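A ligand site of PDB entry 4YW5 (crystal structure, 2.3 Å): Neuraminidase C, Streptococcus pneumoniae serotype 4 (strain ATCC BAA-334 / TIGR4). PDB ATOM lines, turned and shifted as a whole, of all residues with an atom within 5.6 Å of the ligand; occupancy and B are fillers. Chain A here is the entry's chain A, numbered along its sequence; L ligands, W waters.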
ATOM      1  N   ARG A 208      -5.488   5.768  -4.576  1.00  0.00           N
ATOM      2  CA  ARG A 208      -5.276   5.013  -3.349  1.00  0.00           C
ATOM      3  C   ARG A 208      -6.633   4.629  -2.788  1.00  0.00           C
ATOM      4  O   ARG A 208      -7.654   5.181  -3.201  1.00  0.00           O
ATOM      5  CB  ARG A 208      -4.502   5.831  -2.310  1.00  0.00           C
ATOM      6  CG  ARG A 208      -2.990   5.728  -2.399  1.00  0.00           C
ATOM      7  CD  ARG A 208      -2.309   5.966  -1.047  1.00  0.00           C
ATOM      8  NE  ARG A 208      -2.765   4.990  -0.075  1.00  0.00           N
ATOM      9  CZ  ARG A 208      -2.554   5.016   1.238  1.00  0.00           C
ATOM     10  NH1 ARG A 208      -1.857   5.994   1.820  1.00  0.00           N
ATOM     11  NH2 ARG A 208      -3.062   4.054   1.995  1.00  0.00           N
ATOM     12  N   ILE A 209      -6.639   3.711  -1.822  1.00  0.00           N
ATOM     13  CA  ILE A 209      -7.851   3.368  -1.053  1.00  0.00           C
ATOM     14  C   ILE A 209      -8.974   2.774  -1.907  1.00  0.00           C
ATOM     15  O   ILE A 209     -10.041   3.345  -1.996  1.00  0.00           O
ATOM     16  CB  ILE A 209      -8.441   4.577  -0.238  1.00  0.00           C
ATOM     17  CG1 ILE A 209      -7.371   5.531   0.302  1.00  0.00           C
ATOM     18  CG2 ILE A 209      -9.302   4.061   0.930  1.00  0.00           C
ATOM     19  CD1 ILE A 209      -6.358   4.914   1.251  1.00  0.00           C
ATOM     20  N   ASP A 225     -10.042   6.504  -3.934  1.00  0.00           N
ATOM     21  CA  ASP A 225      -9.568   7.871  -3.903  1.00  0.00           C
ATOM     22  C   ASP A 225      -8.820   8.163  -5.203  1.00  0.00           C
ATOM     23  O   ASP A 225      -7.904   7.427  -5.574  1.00  0.00           O
ATOM     24  CB  ASP A 225      -8.540   8.127  -2.822  1.00  0.00           C
ATOM     25  CG  ASP A 225      -9.122   8.222  -1.434  1.00  0.00           C
ATOM     26  OD1 ASP A 225     -10.255   7.747  -1.157  1.00  0.00           O
ATOM     27  OD2 ASP A 225      -8.384   8.779  -0.588  1.00  0.00           O
ATOM     28  N   ARG A 227      -6.309  10.803  -6.230  1.00  0.00           N
ATOM     29  CA  ARG A 227      -5.413  11.723  -5.533  1.00  0.00           C
ATOM     30  C   ARG A 227      -4.579  12.431  -6.573  1.00  0.00           C
ATOM     31  O   ARG A 227      -3.848  11.791  -7.314  1.00  0.00           O
ATOM     32  CB  ARG A 227      -4.540  10.972  -4.540  1.00  0.00           C
ATOM     33  CG  ARG A 227      -5.354  10.092  -3.606  1.00  0.00           C
ATOM     34  CD  ARG A 227      -4.570   9.700  -2.373  1.00  0.00           C
ATOM     35  NE  ARG A 227      -5.433   9.208  -1.292  1.00  0.00           N
ATOM     36  CZ  ARG A 227      -5.013   8.937  -0.052  1.00  0.00           C
ATOM     37  NH1 ARG A 227      -3.730   9.080   0.278  1.00  0.00           N
ATOM     38  NH2 ARG A 227      -5.886   8.526   0.858  1.00  0.00           N
ATOM     39  N   ASP A 233      -1.990  11.736   1.670  1.00  0.00           N
ATOM     40  CA  ASP A 233      -3.296  11.930   2.290  1.00  0.00           C
ATOM     41  C   ASP A 233      -3.592  13.400   2.483  1.00  0.00           C
ATOM     42  O   ASP A 233      -4.715  13.836   2.340  1.00  0.00           O
ATOM     43  CB  ASP A 233      -3.421  11.183   3.620  1.00  0.00           C
ATOM     44  CG  ASP A 233      -3.754   9.732   3.423  1.00  0.00           C
ATOM     45  OD1 ASP A 233      -2.831   8.942   3.126  1.00  0.00           O
ATOM     46  OD2 ASP A 233      -4.966   9.388   3.493  1.00  0.00           O
ATOM     47  N   PHE A 234      -2.577  14.145   2.847  1.00  0.00           N
ATOM     48  CA  PHE A 234      -2.717  15.577   3.023  1.00  0.00           C
ATOM     49  C   PHE A 234      -1.327  16.240   2.870  1.00  0.00           C
ATOM     50  O   PHE A 234      -0.312  15.578   3.074  1.00  0.00           O
ATOM     51  CB  PHE A 234      -3.244  15.854   4.431  1.00  0.00           C
ATOM     52  CG  PHE A 234      -2.277  15.439   5.530  1.00  0.00           C
ATOM     53  CD1 PHE A 234      -1.212  16.293   5.923  1.00  0.00           C
ATOM     54  CD2 PHE A 234      -2.390  14.186   6.146  1.00  0.00           C
ATOM     55  CE1 PHE A 234      -0.297  15.907   6.902  1.00  0.00           C
ATOM     56  CE2 PHE A 234      -1.476  13.799   7.124  1.00  0.00           C
ATOM     57  CZ  PHE A 234      -0.441  14.652   7.505  1.00  0.00           C
ATOM     58  N   ILE A 289     -12.454  11.698   1.088  1.00  0.00           N
ATOM     59  CA  ILE A 289     -11.425  10.694   1.282  1.00  0.00           C
ATOM     60  C   ILE A 289     -11.959   9.499   2.044  1.00  0.00           C
ATOM     61  O   ILE A 289     -12.817   9.671   2.900  1.00  0.00           O
ATOM     62  CB  ILE A 289     -10.184  11.345   1.959  1.00  0.00           C
ATOM     63  CG1 ILE A 289      -9.108  10.339   2.307  1.00  0.00           C
ATOM     64  CG2 ILE A 289     -10.573  12.092   3.233  1.00  0.00           C
ATOM     65  CD1 ILE A 289      -7.793  11.006   2.667  1.00  0.00           C
ATOM     66  N   ASP A 290     -11.482   8.306   1.711  1.00  0.00           N
ATOM     67  CA  ASP A 290     -11.712   7.057   2.503  1.00  0.00           C
ATOM     68  C   ASP A 290     -13.185   6.622   2.493  1.00  0.00           C
ATOM     69  O   ASP A 290     -13.929   6.817   3.451  1.00  0.00           O
ATOM     70  CB  ASP A 290     -11.204   7.210   3.954  1.00  0.00           C
ATOM     71  CG  ASP A 290      -9.670   7.195   4.062  1.00  0.00           C
ATOM     72  OD1 ASP A 290      -9.014   6.812   3.091  1.00  0.00           O
ATOM     73  OD2 ASP A 290      -9.097   7.564   5.113  1.00  0.00           O
ATOM     74  N   ASP A 306     -15.132  10.603   4.312  1.00  0.00           N
ATOM     75  CA  ASP A 306     -14.675  11.743   5.137  1.00  0.00           C
ATOM     76  C   ASP A 306     -14.711  12.975   4.256  1.00  0.00           C
ATOM     77  O   ASP A 306     -14.385  12.905   3.080  1.00  0.00           O
ATOM     78  CB  ASP A 306     -13.211  11.580   5.604  1.00  0.00           C
ATOM     79  CG  ASP A 306     -12.961  10.343   6.457  1.00  0.00           C
ATOM     80  OD1 ASP A 306     -13.881   9.620   6.861  1.00  0.00           O
ATOM     81  OD2 ASP A 306     -11.772  10.108   6.745  1.00  0.00           O
ATOM     82  N   MET A 308     -13.341  17.046   4.157  1.00  0.00           N
ATOM     83  CA  MET A 308     -12.409  17.978   4.746  1.00  0.00           C
ATOM     84  C   MET A 308     -12.487  19.271   3.983  1.00  0.00           C
ATOM     85  O   MET A 308     -12.410  19.270   2.742  1.00  0.00           O
ATOM     86  CB  MET A 308     -10.995  17.477   4.623  1.00  0.00           C
ATOM     87  CG  MET A 308     -10.804  16.026   5.014  1.00  0.00           C
ATOM     88  SD  MET A 308     -10.338  15.906   6.735  1.00  0.00           S
ATOM     89  CE  MET A 308      -9.952  14.143   6.717  1.00  0.00           C
ATOM     90  N   PHE A 314      -6.035  15.849   8.834  1.00  0.00           N
ATOM     91  CA  PHE A 314      -6.264  15.198  10.141  1.00  0.00           C
ATOM     92  C   PHE A 314      -5.446  15.890  11.265  1.00  0.00           C
ATOM     93  O   PHE A 314      -5.888  15.935  12.411  1.00  0.00           O
ATOM     94  CB  PHE A 314      -6.037  13.657  10.086  1.00  0.00           C
ATOM     95  CG  PHE A 314      -4.742  13.181  10.719  1.00  0.00           C
ATOM     96  CD1 PHE A 314      -4.684  12.856  12.091  1.00  0.00           C
ATOM     97  CD2 PHE A 314      -3.587  13.030   9.954  1.00  0.00           C
ATOM     98  CE1 PHE A 314      -3.492  12.418  12.673  1.00  0.00           C
ATOM     99  CE2 PHE A 314      -2.384  12.600  10.537  1.00  0.00           C
ATOM    100  CZ  PHE A 314      -2.341  12.299  11.903  1.00  0.00           C
ATOM    101  N   TYR A 451     -13.065   9.277  11.851  1.00  0.00           N
ATOM    102  CA  TYR A 451     -12.517   8.968  10.551  1.00  0.00           C
ATOM    103  C   TYR A 451     -13.002   7.591  10.144  1.00  0.00           C
ATOM    104  O   TYR A 451     -12.917   6.643  10.929  1.00  0.00           O
ATOM    105  CB  TYR A 451     -10.993   9.001  10.626  1.00  0.00           C
ATOM    106  CG  TYR A 451     -10.475  10.344  11.080  1.00  0.00           C
ATOM    107  CD1 TYR A 451     -10.356  11.381  10.199  1.00  0.00           C
ATOM    108  CD2 TYR A 451     -10.180  10.595  12.432  1.00  0.00           C
ATOM    109  CE1 TYR A 451      -9.924  12.644  10.606  1.00  0.00           C
ATOM    110  CE2 TYR A 451      -9.730  11.843  12.848  1.00  0.00           C
ATOM    111  CZ  TYR A 451      -9.603  12.865  11.924  1.00  0.00           C
ATOM    112  OH  TYR A 451      -9.150  14.122  12.281  1.00  0.00           O
ATOM    113  N   TYR A 471     -13.119   5.488  13.479  1.00  0.00           N
ATOM    114  CA  TYR A 471     -12.160   5.600  14.575  1.00  0.00           C
ATOM    115  C   TYR A 471     -11.774   7.066  14.807  1.00  0.00           C
ATOM    116  O   TYR A 471     -11.960   7.903  13.929  1.00  0.00           O
ATOM    117  CB  TYR A 471     -10.910   4.763  14.300  1.00  0.00           C
ATOM    118  CG  TYR A 471     -10.105   5.258  13.146  1.00  0.00           C
ATOM    119  CD1 TYR A 471     -10.506   5.000  11.837  1.00  0.00           C
ATOM    120  CD2 TYR A 471      -8.949   6.024  13.339  1.00  0.00           C
ATOM    121  CE1 TYR A 471      -9.788   5.478  10.756  1.00  0.00           C
ATOM    122  CE2 TYR A 471      -8.221   6.502  12.248  1.00  0.00           C
ATOM    123  CZ  TYR A 471      -8.647   6.224  10.966  1.00  0.00           C
ATOM    124  OH  TYR A 471      -7.963   6.681   9.869  1.00  0.00           O
ATOM    125  N   SER A 500      -4.656   3.770  14.814  1.00  0.00           N
ATOM    126  CA  SER A 500      -5.379   4.217  13.612  1.00  0.00           C
ATOM    127  C   SER A 500      -6.352   3.113  13.248  1.00  0.00           C
ATOM    128  O   SER A 500      -6.106   2.361  12.309  1.00  0.00           O
ATOM    129  CB  SER A 500      -4.407   4.524  12.460  1.00  0.00           C
ATOM    130  OG  SER A 500      -3.585   5.633  12.786  1.00  0.00           O
ATOM    131  N   GLU A 502      -8.666   1.494  11.674  1.00  0.00           N
ATOM    132  CA  GLU A 502      -9.459   1.177  10.496  1.00  0.00           C
ATOM    133  C   GLU A 502      -9.931  -0.248  10.690  1.00  0.00           C
ATOM    134  O   GLU A 502      -9.109  -1.165  10.915  1.00  0.00           O
ATOM    135  CB  GLU A 502      -8.610   1.310   9.229  1.00  0.00           C
ATOM    136  CG  GLU A 502      -8.136   2.739   8.944  1.00  0.00           C
ATOM    137  CD  GLU A 502      -6.926   2.788   8.020  1.00  0.00           C
ATOM    138  OE1 GLU A 502      -5.999   1.988   8.228  1.00  0.00           O
ATOM    139  OE2 GLU A 502      -6.893   3.642   7.097  1.00  0.00           O
ATOM    140  N   ARG A 518      -6.844  -2.426  12.440  1.00  0.00           N
ATOM    141  CA  ARG A 518      -5.453  -1.991  12.486  1.00  0.00           C
ATOM    142  C   ARG A 518      -5.123  -1.455  13.882  1.00  0.00           C
ATOM    143  O   ARG A 518      -5.960  -0.849  14.521  1.00  0.00           O
ATOM    144  CB  ARG A 518      -5.250  -0.918  11.412  1.00  0.00           C
ATOM    145  CG  ARG A 518      -3.906  -0.208  11.406  1.00  0.00           C
ATOM    146  CD  ARG A 518      -3.925   0.821  10.292  1.00  0.00           C
ATOM    147  NE  ARG A 518      -2.713   1.622  10.200  1.00  0.00           N
ATOM    148  CZ  ARG A 518      -2.503   2.546   9.267  1.00  0.00           C
ATOM    149  NH1 ARG A 518      -3.424   2.802   8.340  1.00  0.00           N
ATOM    150  NH2 ARG A 518      -1.343   3.252   9.259  1.00  0.00           N
ATOM    151  N   GLY A 551       1.146  -0.133  11.086  1.00  0.00           N
ATOM    152  CA  GLY A 551       0.019  -0.947  10.645  1.00  0.00           C
ATOM    153  C   GLY A 551      -0.456  -0.617   9.228  1.00  0.00           C
ATOM    154  O   GLY A 551       0.014   0.329   8.617  1.00  0.00           O
ATOM    155  N   ARG A 580       5.033  -2.626   3.912  1.00  0.00           N
ATOM    156  CA  ARG A 580       3.737  -3.067   3.405  1.00  0.00           C
ATOM    157  C   ARG A 580       4.009  -3.979   2.211  1.00  0.00           C
ATOM    158  O   ARG A 580       4.060  -3.533   1.045  1.00  0.00           O
ATOM    159  CB  ARG A 580       2.817  -1.888   3.082  1.00  0.00           C
ATOM    160  CG  ARG A 580       2.411  -1.080   4.314  1.00  0.00           C
ATOM    161  CD  ARG A 580       1.433   0.067   4.003  1.00  0.00           C
ATOM    162  NE  ARG A 580       0.781   0.608   5.200  1.00  0.00           N
ATOM    163  CZ  ARG A 580       0.086   1.742   5.268  1.00  0.00           C
ATOM    164  NH1 ARG A 580      -0.070   2.545   4.184  1.00  0.00           N
ATOM    165  NH2 ARG A 580      -0.467   2.106   6.424  1.00  0.00           N
ATOM    166  N   TYR A 613      -3.198  -1.195   1.069  1.00  0.00           N
ATOM    167  CA  TYR A 613      -4.635  -1.256   1.320  1.00  0.00           C
ATOM    168  C   TYR A 613      -5.288  -2.228   0.326  1.00  0.00           C
ATOM    169  O   TYR A 613      -4.800  -2.406  -0.817  1.00  0.00           O
ATOM    170  CB  TYR A 613      -5.294   0.137   1.206  1.00  0.00           C
ATOM    171  CG  TYR A 613      -5.134   1.021   2.442  1.00  0.00           C
ATOM    172  CD1 TYR A 613      -3.945   1.056   3.165  1.00  0.00           C
ATOM    173  CD2 TYR A 613      -6.219   1.794   2.909  1.00  0.00           C
ATOM    174  CE1 TYR A 613      -3.825   1.836   4.323  1.00  0.00           C
ATOM    175  CE2 TYR A 613      -6.118   2.572   4.044  1.00  0.00           C
ATOM    176  CZ  TYR A 613      -4.921   2.597   4.757  1.00  0.00           C
ATOM    177  OH  TYR A 613      -4.804   3.399   5.846  1.00  0.00           O
ATOM    178  N   SER A 633       2.380   1.885   0.350  1.00  0.00           N
ATOM    179  CA  SER A 633       1.793   3.212   0.433  1.00  0.00           C
ATOM    180  C   SER A 633       2.167   3.998   1.697  1.00  0.00           C
ATOM    181  O   SER A 633       1.691   5.123   1.878  1.00  0.00           O
ATOM    182  CB  SER A 633       0.273   3.135   0.302  1.00  0.00           C
ATOM    183  OG  SER A 633      -0.335   2.440   1.377  1.00  0.00           O
ATOM    184  N   TRP A 634       3.005   3.412   2.540  1.00  0.00           N
ATOM    185  CA  TRP A 634       3.567   4.097   3.689  1.00  0.00           C
ATOM    186  C   TRP A 634       4.975   4.625   3.395  1.00  0.00           C
ATOM    187  O   TRP A 634       5.308   5.741   3.754  1.00  0.00           O
ATOM    188  CB  TRP A 634       3.629   3.148   4.897  1.00  0.00           C
ATOM    189  CG  TRP A 634       4.073   3.827   6.170  1.00  0.00           C
ATOM    190  CD1 TRP A 634       5.325   3.796   6.715  1.00  0.00           C
ATOM    191  CD2 TRP A 634       3.257   4.581   7.075  1.00  0.00           C
ATOM    192  NE1 TRP A 634       5.338   4.497   7.915  1.00  0.00           N
ATOM    193  CE2 TRP A 634       4.085   5.003   8.129  1.00  0.00           C
ATOM    194  CE3 TRP A 634       1.904   4.956   7.072  1.00  0.00           C
ATOM    195  CZ2 TRP A 634       3.607   5.782   9.180  1.00  0.00           C
ATOM    196  CZ3 TRP A 634       1.436   5.728   8.092  1.00  0.00           C
ATOM    197  CH2 TRP A 634       2.291   6.134   9.155  1.00  0.00           C
HETATM  198  C1  LIG L   1      -2.199   5.136   5.632  1.00  0.00           C
HETATM  199  O1  LIG L   1      -1.908   4.889   4.447  1.00  0.00           O
HETATM  200  O2  LIG L   1      -1.531   4.632   6.548  1.00  0.00           O
HETATM  201  C2  LIG L   1      -3.335   5.993   5.967  1.00  0.00           C
HETATM  202  C3  LIG L   1      -4.327   6.330   4.875  1.00  0.00           C
HETATM  203  C4  LIG L   1      -5.630   6.886   5.418  1.00  0.00           C
HETATM  204  C5  LIG L   1      -5.349   7.949   6.485  1.00  0.00           C
HETATM  205  N1  LIG L   1      -6.572   8.585   6.944  1.00  0.00           N
HETATM  206  C6  LIG L   1      -6.768   9.922   7.012  1.00  0.00           C
HETATM  207  O3  LIG L   1      -5.960  10.754   6.637  1.00  0.00           O
HETATM  208  C7  LIG L   1      -8.055  10.414   7.617  1.00  0.00           C
HETATM  209  C8  LIG L   1      -4.586   7.343   7.665  1.00  0.00           C
HETATM  210  C9  LIG L   1      -3.467   6.435   7.220  1.00  0.00           C
HETATM  211  O4  LIG L   1      -3.946   8.408   8.349  1.00  0.00           O
HETATM  212  C10 LIG L   1      -3.875   8.565   9.784  1.00  0.00           C
HETATM  213  C11 LIG L   1      -5.200   8.316  10.489  1.00  0.00           C
HETATM  214  C12 LIG L   1      -2.779   7.699  10.388  1.00  0.00           C
HETATM  215  C13 LIG L   1      -1.409   8.168   9.931  1.00  0.00           C
HETATM  216  C14 LIG L   1      -5.322   9.263  11.667  1.00  0.00           C
HETATM  217  N2  LIG L   1      -6.407   7.438   4.331  1.00  0.00           N
HETATM  218  O   HOH W   1      -3.235  10.823   7.355  1.00  0.00           O
HETATM  219  O   HOH W   2      -8.189   6.052   7.391  1.00  0.00           O
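OD2 of Asp 290 lies within salt-bridge range of N2 of the ligand, 2.8 Å away. An oxygen (O1) of the ligand is in salt-bridge range of the guanidinium group (NH2) of Arg 208 (2.8 Å). O2 of the ligand is in salt-bridge range of NH2 of Arg 518, 3.0 Å away. OD2 of Asp 233 is in salt-bridge range of N2 of the ligand (2.6 Å). NH2 of Arg 580 is in salt-bridge range of O2 of the ligand (2.7 Å).
N of Asp 225 sits at hydrogen-bond distance from O of Arg 208. The guanidinium group of Arg 518 sits at hydrogen-bond distance from the side-chain hydroxyl of Tyr 613, at 2.9 Å. The side-chain carboxylate of Glu 502 is in hydrogen-bond range of the side-chain hydroxyl of Tyr 613, 2.4 Å away. The backbone carbonyl oxygen of Gly 551 is in hydrogen-bond range of the guanidinium group of Arg 580 (2.9 Å). The backbone NH (N) of Asp 290 is in hydrogen-bond range of the side-chain carboxylate (OD1) of Asp 225. The side-chain carboxylate (OD2) of Asp 225 is in salt-bridge range of the guanidinium group (NH2) of Arg 227 (2.9 Å). NH2 of Arg 208 is in hydrogen-bond range of OG of Ser 633, 3.2 Å away. NH2 of Arg 227 is in salt-bridge range of OD2 of Asp 233, at 2.9 Å.
Residues that only touch the ligand: Tyr 613 (3.0 Å), Ser 500 (3.3 Å), Tyr 471 (3.3 Å), Trp 634 (3.5 Å), Tyr 451 (3.6 Å), Phe 314 (3.7 Å), Arg 227 (3.7 Å), Asp 306 (3.8 Å), Glu 502 (3.9 Å) and Ile 209 (3.98 Å). Of the 21 residues printed, 15 come within 4 Å of the ligand. The nearest printed residue that does not touch the ligand is Ile 289 (4.2 Å).
Water W2 lies within hydrogen-bond range of OH of Tyr 471 (2.6 Å), OE2 of Glu 502 (2.8 Å), OD2 of Asp 290 (2.9 Å) and N1 of the ligand (3.0 Å).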
